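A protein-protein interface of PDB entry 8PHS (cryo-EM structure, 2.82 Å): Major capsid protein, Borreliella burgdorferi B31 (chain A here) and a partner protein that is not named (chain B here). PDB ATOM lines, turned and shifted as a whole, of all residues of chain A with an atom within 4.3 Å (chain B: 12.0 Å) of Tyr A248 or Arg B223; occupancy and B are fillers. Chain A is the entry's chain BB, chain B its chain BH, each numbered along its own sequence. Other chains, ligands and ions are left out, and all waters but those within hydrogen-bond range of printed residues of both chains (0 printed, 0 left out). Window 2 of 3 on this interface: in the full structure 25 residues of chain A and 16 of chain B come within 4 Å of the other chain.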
ATOM      1  N   LYS A  27      16.365 -23.191  25.609  1.00  0.00           N
ATOM      2  CA  LYS A  27      16.653 -24.228  26.590  1.00  0.00           C
ATOM      3  C   LYS A  27      16.284 -23.819  28.009  1.00  0.00           C
ATOM      4  O   LYS A  27      16.407 -24.638  28.924  1.00  0.00           O
ATOM      5  CB  LYS A  27      18.135 -24.606  26.529  1.00  0.00           C
ATOM      6  CG  LYS A  27      18.587 -25.075  25.156  1.00  0.00           C
ATOM      7  CD  LYS A  27      20.044 -24.734  24.896  1.00  0.00           C
ATOM      8  CE  LYS A  27      20.961 -25.350  25.934  1.00  0.00           C
ATOM      9  NZ  LYS A  27      22.389 -25.052  25.638  1.00  0.00           N
ATOM     10  N   PHE A  29      13.175 -22.708  28.797  1.00  0.00           N
ATOM     11  CA  PHE A  29      11.724 -22.732  28.888  1.00  0.00           C
ATOM     12  C   PHE A  29      11.203 -24.069  28.382  1.00  0.00           C
ATOM     13  O   PHE A  29      11.869 -24.771  27.618  1.00  0.00           O
ATOM     14  CB  PHE A  29      11.092 -21.591  28.080  1.00  0.00           C
ATOM     15  CG  PHE A  29      11.445 -20.223  28.583  1.00  0.00           C
ATOM     16  CD1 PHE A  29      10.849 -19.712  29.720  1.00  0.00           C
ATOM     17  CD2 PHE A  29      12.382 -19.450  27.919  1.00  0.00           C
ATOM     18  CE1 PHE A  29      11.175 -18.454  30.184  1.00  0.00           C
ATOM     19  CE2 PHE A  29      12.712 -18.193  28.378  1.00  0.00           C
ATOM     20  CZ  PHE A  29      12.108 -17.694  29.512  1.00  0.00           C
ATOM     21  N   PRO A 200       8.515 -29.385  36.854  1.00  0.00           N
ATOM     22  CA  PRO A 200       9.978 -29.405  36.752  1.00  0.00           C
ATOM     23  C   PRO A 200      10.569 -28.038  37.060  1.00  0.00           C
ATOM     24  O   PRO A 200       9.928 -27.002  36.873  1.00  0.00           O
ATOM     25  CB  PRO A 200      10.231 -29.809  35.295  1.00  0.00           C
ATOM     26  CG  PRO A 200       8.979 -30.492  34.866  1.00  0.00           C
ATOM     27  CD  PRO A 200       7.870 -29.804  35.599  1.00  0.00           C
ATOM     28  N   MET A 201      11.808 -28.043  37.541  1.00  0.00           N
ATOM     29  CA  MET A 201      12.484 -26.817  37.938  1.00  0.00           C
ATOM     30  C   MET A 201      13.753 -26.619  37.119  1.00  0.00           C
ATOM     31  O   MET A 201      14.372 -27.582  36.654  1.00  0.00           O
ATOM     32  CB  MET A 201      12.822 -26.828  39.432  1.00  0.00           C
ATOM     33  CG  MET A 201      11.612 -27.004  40.328  1.00  0.00           C
ATOM     34  SD  MET A 201      10.685 -25.483  40.595  1.00  0.00           S
ATOM     35  CE  MET A 201      11.954 -24.426  41.282  1.00  0.00           C
ATOM     36  N   MET A 202      14.135 -25.354  36.950  1.00  0.00           N
ATOM     37  CA  MET A 202      15.301 -24.974  36.167  1.00  0.00           C
ATOM     38  C   MET A 202      16.195 -24.079  37.011  1.00  0.00           C
ATOM     39  O   MET A 202      15.707 -23.163  37.687  1.00  0.00           O
ATOM     40  CB  MET A 202      14.889 -24.257  34.876  1.00  0.00           C
ATOM     41  CG  MET A 202      16.020 -23.528  34.172  1.00  0.00           C
ATOM     42  SD  MET A 202      17.258 -24.645  33.491  1.00  0.00           S
ATOM     43  CE  MET A 202      16.329 -25.400  32.162  1.00  0.00           C
ATOM     44  N   VAL A 203      17.497 -24.355  36.966  1.00  0.00           N
ATOM     45  CA  VAL A 203      18.515 -23.609  37.692  1.00  0.00           C
ATOM     46  C   VAL A 203      19.547 -23.119  36.687  1.00  0.00           C
ATOM     47  O   VAL A 203      19.967 -23.870  35.802  1.00  0.00           O
ATOM     48  CB  VAL A 203      19.189 -24.474  38.778  1.00  0.00           C
ATOM     49  CG1 VAL A 203      20.178 -23.648  39.583  1.00  0.00           C
ATOM     50  CG2 VAL A 203      18.146 -25.100  39.679  1.00  0.00           C
ATOM     51  N   ASP A 246      11.672 -33.427  37.732  1.00  0.00           N
ATOM     52  CA  ASP A 246      12.944 -33.152  37.081  1.00  0.00           C
ATOM     53  C   ASP A 246      13.495 -31.790  37.487  1.00  0.00           C
ATOM     54  O   ASP A 246      12.759 -30.804  37.594  1.00  0.00           O
ATOM     55  CB  ASP A 246      12.785 -33.220  35.565  1.00  0.00           C
ATOM     56  CG  ASP A 246      12.352 -34.590  35.090  1.00  0.00           C
ATOM     57  OD1 ASP A 246      13.068 -35.572  35.375  1.00  0.00           O
ATOM     58  OD2 ASP A 246      11.294 -34.687  34.433  1.00  0.00           O
ATOM     59  N   VAL A 247      14.805 -31.749  37.720  1.00  0.00           N
ATOM     60  CA  VAL A 247      15.529 -30.520  38.007  1.00  0.00           C
ATOM     61  C   VAL A 247      16.661 -30.412  36.998  1.00  0.00           C
ATOM     62  O   VAL A 247      17.530 -31.291  36.942  1.00  0.00           O
ATOM     63  CB  VAL A 247      16.081 -30.493  39.442  1.00  0.00           C
ATOM     64  CG1 VAL A 247      16.954 -29.268  39.651  1.00  0.00           C
ATOM     65  CG2 VAL A 247      14.943 -30.521  40.445  1.00  0.00           C
ATOM     66  N   TYR A 248      16.652 -29.348  36.203  1.00  0.00           N
ATOM     67  CA  TYR A 248      17.655 -29.133  35.172  1.00  0.00           C
ATOM     68  C   TYR A 248      18.620 -28.045  35.616  1.00  0.00           C
ATOM     69  O   TYR A 248      18.212 -27.056  36.233  1.00  0.00           O
ATOM     70  CB  TYR A 248      16.999 -28.754  33.844  1.00  0.00           C
ATOM     71  CG  TYR A 248      15.894 -29.700  33.437  1.00  0.00           C
ATOM     72  CD1 TYR A 248      16.166 -31.031  33.152  1.00  0.00           C
ATOM     73  CD2 TYR A 248      14.579 -29.268  33.347  1.00  0.00           C
ATOM     74  CE1 TYR A 248      15.161 -31.901  32.784  1.00  0.00           C
ATOM     75  CE2 TYR A 248      13.568 -30.131  32.979  1.00  0.00           C
ATOM     76  CZ  TYR A 248      13.864 -31.446  32.699  1.00  0.00           C
ATOM     77  OH  TYR A 248      12.860 -32.312  32.331  1.00  0.00           O
ATOM     78  N   ILE A 249      19.902 -28.241  35.319  1.00  0.00           N
ATOM     79  CA  ILE A 249      20.959 -27.308  35.690  1.00  0.00           C
ATOM     80  C   ILE A 249      21.632 -26.818  34.417  1.00  0.00           C
ATOM     81  O   ILE A 249      22.001 -27.624  33.554  1.00  0.00           O
ATOM     82  CB  ILE A 249      21.985 -27.955  36.637  1.00  0.00           C
ATOM     83  CG1 ILE A 249      21.284 -28.533  37.867  1.00  0.00           C
ATOM     84  CG2 ILE A 249      23.040 -26.942  37.052  1.00  0.00           C
ATOM     85  CD1 ILE A 249      22.231 -28.973  38.959  1.00  0.00           C
ATOM     86  N   GLU A 250      21.790 -25.502  34.302  1.00  0.00           N
ATOM     87  CA  GLU A 250      22.394 -24.875  33.140  1.00  0.00           C
ATOM     88  C   GLU A 250      23.429 -23.857  33.593  1.00  0.00           C
ATOM     89  O   GLU A 250      23.307 -23.252  34.662  1.00  0.00           O
ATOM     90  CB  GLU A 250      21.340 -24.183  32.267  1.00  0.00           C
ATOM     91  CG  GLU A 250      20.389 -25.132  31.561  1.00  0.00           C
ATOM     92  CD  GLU A 250      20.869 -25.522  30.180  1.00  0.00           C
ATOM     93  OE1 GLU A 250      21.917 -25.003  29.744  1.00  0.00           O
ATOM     94  OE2 GLU A 250      20.197 -26.348  29.529  1.00  0.00           O
ATOM     95  N   LEU A 264       9.377 -24.539  35.457  1.00  0.00           N
ATOM     96  CA  LEU A 264       9.000 -24.583  34.045  1.00  0.00           C
ATOM     97  C   LEU A 264       7.506 -24.844  33.877  1.00  0.00           C
ATOM     98  O   LEU A 264       7.092 -25.762  33.173  1.00  0.00           O
ATOM     99  CB  LEU A 264       9.824 -25.642  33.322  1.00  0.00           C
ATOM    100  CG  LEU A 264      11.339 -25.436  33.287  1.00  0.00           C
ATOM    101  CD1 LEU A 264      12.002 -26.517  32.453  1.00  0.00           C
ATOM    102  CD2 LEU A 264      11.680 -24.057  32.750  1.00  0.00           C
ATOM    103  N   ARG B 214      11.406 -23.271  15.961  1.00  0.00           N
ATOM    104  CA  ARG B 214      11.306 -23.421  17.412  1.00  0.00           C
ATOM    105  C   ARG B 214      10.568 -24.702  17.785  1.00  0.00           C
ATOM    106  O   ARG B 214      10.988 -25.434  18.694  1.00  0.00           O
ATOM    107  CB  ARG B 214      10.605 -22.208  18.017  1.00  0.00           C
ATOM    108  CG  ARG B 214      10.439 -22.270  19.523  1.00  0.00           C
ATOM    109  CD  ARG B 214       9.630 -21.089  20.016  1.00  0.00           C
ATOM    110  NE  ARG B 214       8.273 -21.112  19.483  1.00  0.00           N
ATOM    111  CZ  ARG B 214       7.493 -20.046  19.373  1.00  0.00           C
ATOM    112  NH1 ARG B 214       7.910 -18.845  19.735  1.00  0.00           N
ATOM    113  NH2 ARG B 214       6.265 -20.189  18.883  1.00  0.00           N
ATOM    114  N   ILE B 215       9.465 -24.989  17.090  1.00  0.00           N
ATOM    115  CA  ILE B 215       8.708 -26.206  17.367  1.00  0.00           C
ATOM    116  C   ILE B 215       9.562 -27.439  17.094  1.00  0.00           C
ATOM    117  O   ILE B 215       9.564 -28.397  17.878  1.00  0.00           O
ATOM    118  CB  ILE B 215       7.404 -26.223  16.548  1.00  0.00           C
ATOM    119  CG1 ILE B 215       6.424 -25.183  17.091  1.00  0.00           C
ATOM    120  CG2 ILE B 215       6.777 -27.605  16.566  1.00  0.00           C
ATOM    121  CD1 ILE B 215       5.142 -25.085  16.301  1.00  0.00           C
ATOM    122  N   GLN B 216      10.304 -27.431  15.986  1.00  0.00           N
ATOM    123  CA  GLN B 216      11.179 -28.554  15.665  1.00  0.00           C
ATOM    124  C   GLN B 216      12.275 -28.723  16.711  1.00  0.00           C
ATOM    125  O   GLN B 216      12.617 -29.852  17.086  1.00  0.00           O
ATOM    126  CB  GLN B 216      11.789 -28.357  14.277  1.00  0.00           C
ATOM    127  CG  GLN B 216      12.659 -29.508  13.810  1.00  0.00           C
ATOM    128  CD  GLN B 216      13.203 -29.292  12.413  1.00  0.00           C
ATOM    129  OE1 GLN B 216      12.891 -28.296  11.760  1.00  0.00           O
ATOM    130  NE2 GLN B 216      14.023 -30.227  11.946  1.00  0.00           N
ATOM    131  N   PHE B 217      12.846 -27.613  17.186  1.00  0.00           N
ATOM    132  CA  PHE B 217      13.873 -27.698  18.217  1.00  0.00           C
ATOM    133  C   PHE B 217      13.322 -28.321  19.489  1.00  0.00           C
ATOM    134  O   PHE B 217      13.975 -29.168  20.109  1.00  0.00           O
ATOM    135  CB  PHE B 217      14.446 -26.315  18.520  1.00  0.00           C
ATOM    136  CG  PHE B 217      15.287 -26.274  19.764  1.00  0.00           C
ATOM    137  CD1 PHE B 217      16.586 -26.749  19.751  1.00  0.00           C
ATOM    138  CD2 PHE B 217      14.773 -25.782  20.952  1.00  0.00           C
ATOM    139  CE1 PHE B 217      17.361 -26.721  20.893  1.00  0.00           C
ATOM    140  CE2 PHE B 217      15.543 -25.757  22.096  1.00  0.00           C
ATOM    141  CZ  PHE B 217      16.839 -26.224  22.065  1.00  0.00           C
ATOM    142  N   TYR B 218      12.123 -27.905  19.904  1.00  0.00           N
ATOM    143  CA  TYR B 218      11.541 -28.491  21.108  1.00  0.00           C
ATOM    144  C   TYR B 218      11.176 -29.956  20.904  1.00  0.00           C
ATOM    145  O   TYR B 218      11.276 -30.753  21.843  1.00  0.00           O
ATOM    146  CB  TYR B 218      10.323 -27.689  21.560  1.00  0.00           C
ATOM    147  CG  TYR B 218      10.687 -26.512  22.432  1.00  0.00           C
ATOM    148  CD1 TYR B 218      11.532 -26.670  23.521  1.00  0.00           C
ATOM    149  CD2 TYR B 218      10.187 -25.245  22.171  1.00  0.00           C
ATOM    150  CE1 TYR B 218      11.872 -25.600  24.322  1.00  0.00           C
ATOM    151  CE2 TYR B 218      10.520 -24.168  22.968  1.00  0.00           C
ATOM    152  CZ  TYR B 218      11.363 -24.353  24.042  1.00  0.00           C
ATOM    153  OH  TYR B 218      11.698 -23.284  24.838  1.00  0.00           O
ATOM    154  N   GLU B 219      10.753 -30.330  19.694  1.00  0.00           N
ATOM    155  CA  GLU B 219      10.474 -31.736  19.415  1.00  0.00           C
ATOM    156  C   GLU B 219      11.741 -32.578  19.495  1.00  0.00           C
ATOM    157  O   GLU B 219      11.714 -33.703  20.008  1.00  0.00           O
ATOM    158  CB  GLU B 219       9.822 -31.881  18.041  1.00  0.00           C
ATOM    159  CG  GLU B 219       8.390 -31.379  17.975  1.00  0.00           C
ATOM    160  CD  GLU B 219       7.810 -31.461  16.577  1.00  0.00           C
ATOM    161  OE1 GLU B 219       8.530 -31.909  15.659  1.00  0.00           O
ATOM    162  OE2 GLU B 219       6.637 -31.078  16.393  1.00  0.00           O
ATOM    163  N   ASN B 220      12.858 -32.056  18.989  1.00  0.00           N
ATOM    164  CA  ASN B 220      14.113 -32.798  19.005  1.00  0.00           C
ATOM    165  C   ASN B 220      14.872 -32.671  20.320  1.00  0.00           C
ATOM    166  O   ASN B 220      15.870 -33.375  20.507  1.00  0.00           O
ATOM    167  CB  ASN B 220      15.016 -32.336  17.859  1.00  0.00           C
ATOM    168  CG  ASN B 220      14.394 -32.570  16.498  1.00  0.00           C
ATOM    169  OD1 ASN B 220      13.301 -33.123  16.388  1.00  0.00           O
ATOM    170  ND2 ASN B 220      15.091 -32.147  15.450  1.00  0.00           N
ATOM    171  N   LEU B 221      14.438 -31.796  21.224  1.00  0.00           N
ATOM    172  CA  LEU B 221      15.150 -31.604  22.478  1.00  0.00           C
ATOM    173  C   LEU B 221      15.028 -32.836  23.368  1.00  0.00           C
ATOM    174  O   LEU B 221      13.970 -33.464  23.447  1.00  0.00           O
ATOM    175  CB  LEU B 221      14.615 -30.374  23.211  1.00  0.00           C
ATOM    176  CG  LEU B 221      15.226 -30.086  24.583  1.00  0.00           C
ATOM    177  CD1 LEU B 221      16.643 -29.556  24.439  1.00  0.00           C
ATOM    178  CD2 LEU B 221      14.362 -29.116  25.366  1.00  0.00           C
ATOM    179  N   LYS B 222      16.126 -33.176  24.041  1.00  0.00           N
ATOM    180  CA  LYS B 222      16.163 -34.298  24.979  1.00  0.00           C
ATOM    181  C   LYS B 222      17.028 -33.878  26.163  1.00  0.00           C
ATOM    182  O   LYS B 222      18.258 -33.841  26.059  1.00  0.00           O
ATOM    183  CB  LYS B 222      16.697 -35.562  24.313  1.00  0.00           C
ATOM    184  CG  LYS B 222      17.793 -35.308  23.290  1.00  0.00           C
ATOM    185  CD  LYS B 222      18.317 -36.605  22.702  1.00  0.00           C
ATOM    186  CE  LYS B 222      19.442 -36.344  21.714  1.00  0.00           C
ATOM    187  NZ  LYS B 222      19.903 -37.594  21.051  1.00  0.00           N
ATOM    188  N   ARG B 223      16.384 -33.552  27.279  1.00  0.00           N
ATOM    189  CA  ARG B 223      17.100 -33.134  28.477  1.00  0.00           C
ATOM    190  C   ARG B 223      17.588 -34.340  29.273  1.00  0.00           C
ATOM    191  O   ARG B 223      18.578 -34.258  30.000  1.00  0.00           O
ATOM    192  CB  ARG B 223      16.213 -32.249  29.356  1.00  0.00           C
ATOM    193  CG  ARG B 223      15.622 -31.043  28.642  1.00  0.00           C
ATOM    194  CD  ARG B 223      14.540 -30.392  29.491  1.00  0.00           C
ATOM    195  NE  ARG B 223      14.064 -29.131  28.935  1.00  0.00           N
ATOM    196  CZ  ARG B 223      14.750 -27.997  28.945  1.00  0.00           C
ATOM    197  NH1 ARG B 223      15.962 -27.924  29.472  1.00  0.00           N
ATOM    198  NH2 ARG B 223      14.206 -26.905  28.417  1.00  0.00           N
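CG of Lys A27 touches CZ of Phe B217, 3.7 Å away.
Met A202 touches Arg B223.
CD of Arg B223 touches CZ of Tyr A248 (3.4 Å).
Hydrophobic or aromatic side chains of chain B within 4 Å of the printed part of chain A: Phe B217 and Tyr B218.
Printed residues of chain A that touch a printed residue of chain B: Lys A27, Phe A29, Met A202 and Tyr A248.
Hydrophobic or aromatic side chains of chain A within 4 Å of the printed part of chain B: Phe A29, Met A202 and Tyr A248.
Among the printed residues, no Asp or Glu carboxylate lies within 4 Å of a Lys or Arg side-chain nitrogen of the other chain.
NH2 of Arg B223 is in hydrogen-bond range of O of Lys A27.
The backbone carbonyl oxygen (O) of Phe A29 is in hydrogen-bond range of the side-chain hydroxyl (OH) of Tyr B218.
The backbone carbonyl oxygen of Phe A29 sits at hydrogen-bond distance from the guanidinium group of Arg B223, at 3.3 Å.
The backbone NH of Tyr A248 sits at hydrogen-bond distance from the backbone carbonyl oxygen of Met A201, at 2.9 Å.
N of Val A203 is in hydrogen-bond range of O of Tyr A248 (2.9 Å).
Printed residues of chain B within 4 Å of Lys A27: Phe B217 and Arg B223.
Of the printed residues of chain B, Phe A29 touches Tyr B218 and Arg B223.
No residue of chain B comes within 4 Å of Pro A200.
Of the printed residues of chain B, Met A202 touches Arg B223.
No residue of chain B comes within 4 Å of Asp A246.
No residue of chain B comes within 4 Å of Val A247.
Of the printed residues of chain B, Tyr A248 touches Arg B223.
Glu A250 touches none of the printed residues of chain B.
Arg B214 touches none of the printed residues of chain A.
Of the printed residues of chain A, Phe B217 touches Lys A27.
Of the printed residues of chain A, Tyr B218 touches Phe A29.
Lys B222 touches none of the printed residues of chain A.
Of chain A, only Lys A27 (3.2 Å), Phe A29 (3.3 Å), Met A202 (3.7 Å) and Tyr A248 (3.4 Å) come within 4 Å of Arg B223.
The nearest residue of chain B that does not touch Tyr A248 is Lys B222 (7.2 Å).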
